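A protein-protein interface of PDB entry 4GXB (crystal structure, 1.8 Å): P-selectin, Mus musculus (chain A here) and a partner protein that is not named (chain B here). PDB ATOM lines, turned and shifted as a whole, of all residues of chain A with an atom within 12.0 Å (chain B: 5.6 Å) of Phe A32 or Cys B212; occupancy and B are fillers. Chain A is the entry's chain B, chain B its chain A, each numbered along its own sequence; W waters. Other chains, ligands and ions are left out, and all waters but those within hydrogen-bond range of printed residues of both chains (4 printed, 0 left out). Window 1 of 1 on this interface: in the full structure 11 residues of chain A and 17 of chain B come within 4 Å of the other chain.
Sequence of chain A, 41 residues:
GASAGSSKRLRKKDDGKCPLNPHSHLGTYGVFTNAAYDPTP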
ATOM      1  N   GLY A  27     -30.819  33.468   6.997  1.00  0.00           N
ATOM      2  CA  GLY A  27     -31.200  34.060   5.727  1.00  0.00           C
ATOM      3  C   GLY A  27     -32.371  33.345   5.078  1.00  0.00           C
ATOM      4  O   GLY A  27     -32.758  32.253   5.509  1.00  0.00           O
ATOM      5  N   THR A  28     -32.937  33.961   4.043  1.00  0.00           N
ATOM      6  CA  THR A  28     -34.077  33.391   3.326  1.00  0.00           C
ATOM      7  C   THR A  28     -33.722  33.006   1.893  1.00  0.00           C
ATOM      8  O   THR A  28     -34.141  31.956   1.397  1.00  0.00           O
ATOM      9  CB  THR A  28     -35.265  34.380   3.293  1.00  0.00           C
ATOM     10  OG1 THR A  28     -35.782  34.546   4.618  1.00  0.00           O
ATOM     11  CG2 THR A  28     -36.368  33.862   2.394  1.00  0.00           C
ATOM     12  N   TYR A  29     -32.951  33.858   1.228  1.00  0.00           N
ATOM     13  CA  TYR A  29     -32.604  33.623  -0.166  1.00  0.00           C
ATOM     14  C   TYR A  29     -31.133  33.277  -0.296  1.00  0.00           C
ATOM     15  O   TYR A  29     -30.345  33.547   0.608  1.00  0.00           O
ATOM     16  CB  TYR A  29     -32.944  34.848  -1.023  1.00  0.00           C
ATOM     17  CG  TYR A  29     -34.404  35.202  -0.969  1.00  0.00           C
ATOM     18  CD1 TYR A  29     -35.313  34.582  -1.809  1.00  0.00           C
ATOM     19  CD2 TYR A  29     -34.879  36.141  -0.064  1.00  0.00           C
ATOM     20  CE1 TYR A  29     -36.651  34.889  -1.753  1.00  0.00           C
ATOM     21  CE2 TYR A  29     -36.223  36.456  -0.001  1.00  0.00           C
ATOM     22  CZ  TYR A  29     -37.102  35.826  -0.852  1.00  0.00           C
ATOM     23  OH  TYR A  29     -38.441  36.127  -0.802  1.00  0.00           O
ATOM     24  N   GLY A  30     -30.771  32.678  -1.425  1.00  0.00           N
ATOM     25  CA  GLY A  30     -29.395  32.298  -1.670  1.00  0.00           C
ATOM     26  C   GLY A  30     -29.149  30.825  -1.384  1.00  0.00           C
ATOM     27  O   GLY A  30     -30.082  30.016  -1.365  1.00  0.00           O
ATOM     28  N   VAL A  31     -27.891  30.486  -1.131  1.00  0.00           N
ATOM     29  CA  VAL A  31     -27.474  29.092  -1.033  1.00  0.00           C
ATOM     30  C   VAL A  31     -27.374  28.610   0.407  1.00  0.00           C
ATOM     31  O   VAL A  31     -26.836  29.296   1.276  1.00  0.00           O
ATOM     32  CB  VAL A  31     -26.122  28.874  -1.740  1.00  0.00           C
ATOM     33  CG1 VAL A  31     -25.724  27.403  -1.697  1.00  0.00           C
ATOM     34  CG2 VAL A  31     -26.209  29.358  -3.182  1.00  0.00           C
ATOM     35  N   PHE A  32     -27.907  27.420   0.664  1.00  0.00           N
ATOM     36  CA  PHE A  32     -27.833  26.832   1.990  1.00  0.00           C
ATOM     37  C   PHE A  32     -26.972  25.579   1.937  1.00  0.00           C
ATOM     38  O   PHE A  32     -27.281  24.654   1.205  1.00  0.00           O
ATOM     39  CB  PHE A  32     -29.233  26.478   2.493  1.00  0.00           C
ATOM     40  CG  PHE A  32     -30.134  27.674   2.655  1.00  0.00           C
ATOM     41  CD1 PHE A  32     -30.739  28.258   1.556  1.00  0.00           C
ATOM     42  CD2 PHE A  32     -30.363  28.217   3.906  1.00  0.00           C
ATOM     43  CE1 PHE A  32     -31.568  29.368   1.700  1.00  0.00           C
ATOM     44  CE2 PHE A  32     -31.194  29.320   4.059  1.00  0.00           C
ATOM     45  CZ  PHE A  32     -31.789  29.895   2.954  1.00  0.00           C
ATOM     46  N   THR A  33     -25.896  25.558   2.714  1.00  0.00           N
ATOM     47  CA  THR A  33     -25.017  24.394   2.768  1.00  0.00           C
ATOM     48  C   THR A  33     -25.665  23.302   3.634  1.00  0.00           C
ATOM     49  O   THR A  33     -26.097  23.565   4.752  1.00  0.00           O
ATOM     50  CB  THR A  33     -23.643  24.777   3.340  1.00  0.00           C
ATOM     51  OG1 THR A  33     -23.047  25.791   2.502  1.00  0.00           O
ATOM     52  CG2 THR A  33     -22.726  23.560   3.384  1.00  0.00           C
ATOM     53  N   ASN A  34     -25.753  22.085   3.112  1.00  0.00           N
ATOM     54  CA  ASN A  34     -26.363  20.989   3.872  1.00  0.00           C
ATOM     55  C   ASN A  34     -25.364  20.267   4.761  1.00  0.00           C
ATOM     56  O   ASN A  34     -24.573  19.454   4.291  1.00  0.00           O
ATOM     57  CB  ASN A  34     -27.036  19.992   2.925  1.00  0.00           C
ATOM     58  CG  ASN A  34     -27.683  18.830   3.669  1.00  0.00           C
ATOM     59  OD1 ASN A  34     -27.821  18.866   4.894  1.00  0.00           O
ATOM     60  ND2 ASN A  34     -28.069  17.793   2.934  1.00  0.00           N
ATOM     61  N   ALA A  35     -25.398  20.551   6.061  1.00  0.00           N
ATOM     62  CA  ALA A  35     -24.477  19.888   6.983  1.00  0.00           C
ATOM     63  C   ALA A  35     -24.608  18.364   6.975  1.00  0.00           C
ATOM     64  O   ALA A  35     -23.659  17.656   7.296  1.00  0.00           O
ATOM     65  CB  ALA A  35     -24.644  20.427   8.402  1.00  0.00           C
ATOM     66  N   ALA A  36     -25.786  17.867   6.603  1.00  0.00           N
ATOM     67  CA  ALA A  36     -26.061  16.432   6.631  1.00  0.00           C
ATOM     68  C   ALA A  36     -25.682  15.686   5.338  1.00  0.00           C
ATOM     69  O   ALA A  36     -25.930  14.479   5.211  1.00  0.00           O
ATOM     70  CB  ALA A  36     -27.549  16.196   6.982  1.00  0.00           C
ATOM     71  N   TYR A  37     -25.082  16.400   4.385  1.00  0.00           N
ATOM     72  CA  TYR A  37     -24.680  15.782   3.122  1.00  0.00           C
ATOM     73  C   TYR A  37     -23.679  14.664   3.378  1.00  0.00           C
ATOM     74  O   TYR A  37     -22.687  14.863   4.069  1.00  0.00           O
ATOM     75  CB  TYR A  37     -24.049  16.831   2.208  1.00  0.00           C
ATOM     76  CG  TYR A  37     -23.573  16.306   0.875  1.00  0.00           C
ATOM     77  CD1 TYR A  37     -24.456  15.731  -0.025  1.00  0.00           C
ATOM     78  CD2 TYR A  37     -22.243  16.440   0.494  1.00  0.00           C
ATOM     79  CE1 TYR A  37     -24.017  15.276  -1.271  1.00  0.00           C
ATOM     80  CE2 TYR A  37     -21.801  15.986  -0.737  1.00  0.00           C
ATOM     81  CZ  TYR A  37     -22.690  15.409  -1.609  1.00  0.00           C
ATOM     82  OH  TYR A  37     -22.242  14.962  -2.827  1.00  0.00           O
ATOM     83  N   ASP A  38     -23.942  13.487   2.822  1.00  0.00           N
ATOM     84  CA  ASP A  38     -23.091  12.320   3.053  1.00  0.00           C
ATOM     85  C   ASP A  38     -22.959  11.523   1.766  1.00  0.00           C
ATOM     86  O   ASP A  38     -23.804  10.683   1.470  1.00  0.00           O
ATOM     87  CB  ASP A  38     -23.704  11.437   4.153  1.00  0.00           C
ATOM     88  CG  ASP A  38     -22.816  10.263   4.528  1.00  0.00           C
ATOM     89  OD1 ASP A  38     -21.683  10.173   4.014  1.00  0.00           O
ATOM     90  OD2 ASP A  38     -23.257   9.422   5.337  1.00  0.00           O
ATOM     91  N   PRO A  39     -21.906  11.802   0.978  1.00  0.00           N
ATOM     92  CA  PRO A  39     -21.765  11.168  -0.339  1.00  0.00           C
ATOM     93  C   PRO A  39     -21.277   9.724  -0.252  1.00  0.00           C
ATOM     94  O   PRO A  39     -21.180   9.061  -1.280  1.00  0.00           O
ATOM     95  CB  PRO A  39     -20.734  12.053  -1.055  1.00  0.00           C
ATOM     96  CG  PRO A  39     -19.946  12.687   0.050  1.00  0.00           C
ATOM     97  CD  PRO A  39     -20.915  12.870   1.198  1.00  0.00           C
ATOM     98  N   MET B 210     -28.256  15.603  -0.806  1.00  0.00           N
ATOM     99  CA  MET B 210     -28.304  16.988  -1.288  1.00  0.00           C
ATOM    100  C   MET B 210     -27.084  17.743  -0.782  1.00  0.00           C
ATOM    101  O   MET B 210     -26.919  17.923   0.425  1.00  0.00           O
ATOM    102  CB  MET B 210     -29.569  17.684  -0.792  1.00  0.00           C
ATOM    103  CG  MET B 210     -30.854  17.053  -1.273  1.00  0.00           C
ATOM    104  SD  MET B 210     -32.311  17.881  -0.563  1.00  0.00           S
ATOM    105  CE  MET B 210     -33.601  16.882  -1.310  1.00  0.00           C
ATOM    106  N   ARG B 211     -26.212  18.177  -1.691  1.00  0.00           N
ATOM    107  CA  ARG B 211     -25.001  18.877  -1.252  1.00  0.00           C
ATOM    108  C   ARG B 211     -25.377  20.261  -0.724  1.00  0.00           C
ATOM    109  O   ARG B 211     -24.830  20.718   0.278  1.00  0.00           O
ATOM    110  CB  ARG B 211     -23.963  18.992  -2.379  1.00  0.00           C
ATOM    111  CG  ARG B 211     -22.589  19.400  -1.865  1.00  0.00           C
ATOM    112  CD  ARG B 211     -21.493  19.326  -2.951  1.00  0.00           C
ATOM    113  NE  ARG B 211     -21.747  20.250  -4.049  1.00  0.00           N
ATOM    114  CZ  ARG B 211     -20.857  20.550  -4.993  1.00  0.00           C
ATOM    115  NH1 ARG B 211     -19.658  19.997  -4.962  1.00  0.00           N
ATOM    116  NH2 ARG B 211     -21.164  21.407  -5.962  1.00  0.00           N
ATOM    117  N   CYS B 212     -26.329  20.897  -1.395  1.00  0.00           N
ATOM    118  CA  CYS B 212     -26.868  22.185  -0.961  1.00  0.00           C
ATOM    119  C   CYS B 212     -28.232  22.444  -1.601  1.00  0.00           C
ATOM    120  O   CYS B 212     -28.704  21.664  -2.428  1.00  0.00           O
ATOM    121  CB  CYS B 212     -25.892  23.311  -1.330  1.00  0.00           C
ATOM    122  SG  CYS B 212     -25.806  23.642  -3.103  1.00  0.00           S
ATOM    123  N   TRP B 213     -28.891  23.530  -1.210  1.00  0.00           N
ATOM    124  CA  TRP B 213     -30.075  23.967  -1.941  1.00  0.00           C
ATOM    125  C   TRP B 213     -30.077  25.485  -1.995  1.00  0.00           C
ATOM    126  O   TRP B 213     -29.364  26.133  -1.246  1.00  0.00           O
ATOM    127  CB  TRP B 213     -31.380  23.429  -1.331  1.00  0.00           C
ATOM    128  CG  TRP B 213     -31.548  23.718   0.135  1.00  0.00           C
ATOM    129  CD1 TRP B 213     -32.126  24.820   0.696  1.00  0.00           C
ATOM    130  CD2 TRP B 213     -31.143  22.877   1.221  1.00  0.00           C
ATOM    131  NE1 TRP B 213     -32.102  24.716   2.077  1.00  0.00           N
ATOM    132  CE2 TRP B 213     -31.502  23.532   2.418  1.00  0.00           C
ATOM    133  CE3 TRP B 213     -30.517  21.631   1.298  1.00  0.00           C
ATOM    134  CZ2 TRP B 213     -31.248  22.986   3.673  1.00  0.00           C
ATOM    135  CZ3 TRP B 213     -30.274  21.084   2.554  1.00  0.00           C
ATOM    136  CH2 TRP B 213     -30.638  21.764   3.717  1.00  0.00           C
ATOM    137  N   ARG B 214     -30.889  26.032  -2.882  1.00  0.00           N
ATOM    138  CA  ARG B 214     -30.885  27.465  -3.121  1.00  0.00           C
ATOM    139  C   ARG B 214     -32.311  27.944  -3.326  1.00  0.00           C
ATOM    140  O   ARG B 214     -33.091  27.315  -4.043  1.00  0.00           O
ATOM    141  CB  ARG B 214     -30.015  27.756  -4.352  1.00  0.00           C
ATOM    142  CG  ARG B 214     -30.077  29.170  -4.891  1.00  0.00           C
ATOM    143  CD  ARG B 214     -29.232  29.303  -6.159  1.00  0.00           C
ATOM    144  NE  ARG B 214     -29.211  28.071  -6.947  1.00  0.00           N
ATOM    145  CZ  ARG B 214     -29.003  28.025  -8.262  1.00  0.00           C
ATOM    146  NH1 ARG B 214     -28.818  29.151  -8.941  1.00  0.00           N
ATOM    147  NH2 ARG B 214     -28.990  26.861  -8.905  1.00  0.00           N
ATOM    148  N   VAL B 215     -32.657  29.069  -2.706  1.00  0.00           N
ATOM    149  CA  VAL B 215     -33.953  29.682  -2.936  1.00  0.00           C
ATOM    150  C   VAL B 215     -33.745  30.973  -3.732  1.00  0.00           C
ATOM    151  O   VAL B 215     -32.931  31.808  -3.351  1.00  0.00           O
ATOM    152  CB  VAL B 215     -34.660  30.017  -1.611  1.00  0.00           C
ATOM    153  CG1 VAL B 215     -35.994  30.701  -1.889  1.00  0.00           C
ATOM    154  CG2 VAL B 215     -34.865  28.738  -0.793  1.00  0.00           C
ATOM    155  N   ALA B 241     -34.109  25.079  -5.603  1.00  0.00           N
ATOM    156  CA  ALA B 241     -33.307  24.162  -6.403  1.00  0.00           C
ATOM    157  C   ALA B 241     -32.389  23.419  -5.449  1.00  0.00           C
ATOM    158  O   ALA B 241     -31.798  24.026  -4.571  1.00  0.00           O
ATOM    159  CB  ALA B 241     -32.498  24.932  -7.434  1.00  0.00           C
ATOM    160  N   PHE B 242     -32.280  22.105  -5.589  1.00  0.00           N
ATOM    161  CA  PHE B 242     -31.331  21.374  -4.749  1.00  0.00           C
ATOM    162  C   PHE B 242     -30.344  20.603  -5.603  1.00  0.00           C
ATOM    163  O   PHE B 242     -30.695  20.108  -6.673  1.00  0.00           O
ATOM    164  CB  PHE B 242     -32.033  20.454  -3.725  1.00  0.00           C
ATOM    165  CG  PHE B 242     -32.941  19.405  -4.339  1.00  0.00           C
ATOM    166  CD1 PHE B 242     -32.446  18.159  -4.709  1.00  0.00           C
ATOM    167  CD2 PHE B 242     -34.285  19.655  -4.514  1.00  0.00           C
ATOM    168  CE1 PHE B 242     -33.288  17.192  -5.266  1.00  0.00           C
ATOM    169  CE2 PHE B 242     -35.133  18.701  -5.064  1.00  0.00           C
ATOM    170  CZ  PHE B 242     -34.631  17.464  -5.439  1.00  0.00           C
ATOM    171  N   GLU B 243     -29.111  20.535  -5.131  1.00  0.00           N
ATOM    172  CA  GLU B 243     -28.035  19.919  -5.905  1.00  0.00           C
ATOM    173  C   GLU B 243     -27.879  18.477  -5.425  1.00  0.00           C
ATOM    174  O   GLU B 243     -27.371  18.225  -4.336  1.00  0.00           O
ATOM    175  CB  GLU B 243     -26.737  20.698  -5.735  1.00  0.00           C
ATOM    176  CG  GLU B 243     -25.714  20.373  -6.817  1.00  0.00           C
ATOM    177  CD  GLU B 243     -24.401  21.098  -6.637  1.00  0.00           C
ATOM    178  OE1 GLU B 243     -24.109  21.568  -5.520  1.00  0.00           O
ATOM    179  OE2 GLU B 243     -23.648  21.171  -7.619  1.00  0.00           O
ATOM    180  N   TRP B 253     -28.682  19.465 -10.501  1.00  0.00           N
ATOM    181  CA  TRP B 253     -29.657  20.375  -9.886  1.00  0.00           C
ATOM    182  C   TRP B 253     -31.091  19.996 -10.245  1.00  0.00           C
ATOM    183  O   TRP B 253     -31.406  19.752 -11.414  1.00  0.00           O
ATOM    184  CB  TRP B 253     -29.384  21.825 -10.307  1.00  0.00           C
ATOM    185  CG  TRP B 253     -28.174  22.439  -9.683  1.00  0.00           C
ATOM    186  CD1 TRP B 253     -26.907  22.481 -10.202  1.00  0.00           C
ATOM    187  CD2 TRP B 253     -28.111  23.114  -8.421  1.00  0.00           C
ATOM    188  NE1 TRP B 253     -26.065  23.143  -9.343  1.00  0.00           N
ATOM    189  CE2 TRP B 253     -26.780  23.541  -8.243  1.00  0.00           C
ATOM    190  CE3 TRP B 253     -29.053  23.395  -7.422  1.00  0.00           C
ATOM    191  CZ2 TRP B 253     -26.366  24.236  -7.108  1.00  0.00           C
ATOM    192  CZ3 TRP B 253     -28.641  24.087  -6.305  1.00  0.00           C
ATOM    193  CH2 TRP B 253     -27.312  24.504  -6.157  1.00  0.00           C
ATOM    194  N   SER B 265     -37.604  24.990   1.757  1.00  0.00           N
ATOM    195  CA  SER B 265     -36.255  25.209   2.240  1.00  0.00           C
ATOM    196  C   SER B 265     -36.197  25.047   3.762  1.00  0.00           C
ATOM    197  O   SER B 265     -35.271  24.439   4.296  1.00  0.00           O
ATOM    198  CB  SER B 265     -35.802  26.630   1.862  1.00  0.00           C
ATOM    199  OG  SER B 265     -34.549  26.911   2.431  1.00  0.00           O
ATOM    200  N   GLN B 269     -33.960  22.293   5.844  1.00  0.00           N
ATOM    201  CA  GLN B 269     -33.059  22.659   6.936  1.00  0.00           C
ATOM    202  C   GLN B 269     -33.428  21.918   8.216  1.00  0.00           C
ATOM    203  O   GLN B 269     -32.564  21.429   8.943  1.00  0.00           O
ATOM    204  CB  GLN B 269     -33.092  24.159   7.220  1.00  0.00           C
ATOM    205  CG  GLN B 269     -32.001  24.570   8.216  1.00  0.00           C
ATOM    206  CD  GLN B 269     -30.606  24.399   7.627  1.00  0.00           C
ATOM    207  OE1 GLN B 269     -30.263  25.040   6.629  1.00  0.00           O
ATOM    208  NE2 GLN B 269     -29.804  23.519   8.228  1.00  0.00           N
HETATM  209  O   HOH W   1     -27.836  25.486   5.956  1.00  0.00           O
HETATM  210  O   HOH W   2     -31.187  34.117  -4.226  1.00  0.00           O
HETATM  211  O   HOH W   3     -27.380  22.227   7.506  1.00  0.00           O
HETATM  212  O   HOH W   4     -35.259  29.786   2.712  1.00  0.00           O
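Of chain B, only Cys B212, Trp B213 and Ser B265 come within 4 Å of Phe A32. Of the printed residues of chain A, Cys B212 touches Phe A32. Met B210 touches just these residues of chain A: Asn A34 (2.8 Å) and Tyr A37 (3.3 Å). Of chain A, only Asn A34 (3.3 Å) and Tyr A37 (3.4 Å) come within 4 Å of Arg B211. Of chain A, only Gly A30 (3.95 Å), Val A31 (3.5 Å), Phe A32 (2.7 Å) and Asn A34 (3.4 Å) come within 4 Å of Trp B213. Val B215 touches just these residues of chain A: Thr A28 (3.6 Å), Tyr A29 (3.7 Å) and Gly A30 (3.0 Å). No residue of chain A comes within 4 Å of Ala B241. No residue of chain A comes within 4 Å of Phe B242. Of the printed residues of chain A, Ser B265 touches Phe A32 (3.9 Å). Of the printed residues of chain A, Arg B214 touches Gly A30 (3.2 Å). Of the printed residues of chain B, Thr A28 touches Val B215. The nearest printed residue of chain A that does not touch Cys B212 is Val A31 (4.02 Å). The nearest printed residue of chain B that does not touch Tyr A37 is Glu B243 (5.4 Å).
The backbone carbonyl oxygen of Met B210 is in hydrogen-bond range of the side-chain amide nitrogen of Asn A34 (2.8 Å). The backbone carbonyl oxygen of Arg B211 sits at hydrogen-bond distance from the backbone NH of Asn A34 (3.3 Å). N of Phe A32 lies within hydrogen-bond range of O of Trp B213, at 2.7 Å. The backbone carbonyl oxygen (O) of Val B215 lies within hydrogen-bond range of the backbone NH (N) of Gly A30.
OE1 of Glu B243 is in salt-bridge range of NH2 of Arg B211 (3.0 Å). The backbone carbonyl oxygen of Cys B212 is in hydrogen-bond range of the backbone NH of Glu B243 (3.0 Å). NE1 of Trp B213 sits at hydrogen-bond distance from OG of Ser B265, 3.3 Å away. N of Arg B214 is in hydrogen-bond range of O of Ala B241, 2.8 Å away. The side-chain amide oxygen (OD1) of Asn A34 is in hydrogen-bond range of the backbone NH (N) of Ala A36 (2.8 Å).
Water W1 lies within hydrogen-bond range of OE1 of Gln B269 and O of Thr A33. Water W4 lies within hydrogen-bond range of the backbone carbonyl oxygen (O) of Thr A28 (2.8 Å) and the side-chain hydroxyl (OG) of Ser B265 (3.0 Å). Water W3 lies within hydrogen-bond range of the side-chain amide nitrogen (NE2) of Gln B269, the backbone NH (N) of Ala A35 and the backbone carbonyl oxygen (O) of Thr A33. Water W2 bridges the backbone carbonyl oxygen (O) of Val B215 (3.0 Å) and the backbone NH (N) of Gly A30 (3.2 Å).
Among the printed residues, merely in contact across the chains: Phe A32 with Cys B212 (3.2 Å), Gly A30 with Arg B214 (3.2 Å), Tyr A37 with Met B210 (3.3 Å), Tyr A37 with Arg B211 (3.4 Å), Asn A34 with Trp B213 (3.4 Å), Val A31 with Trp B213 (3.5 Å), Thr A28 with Val B215 (3.6 Å), Tyr A29 with Val B215 (3.7 Å), Phe A32 with Ser B265 (3.9 Å) and Gly A30 with Trp B213 (3.95 Å).
Of the 13 printed residues of chain A, 7 touch a printed residue of chain B. Of the 12 printed residues of chain B, 7 touch a printed residue of chain A. Among the printed residues, 14 pairs touch across the chains.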
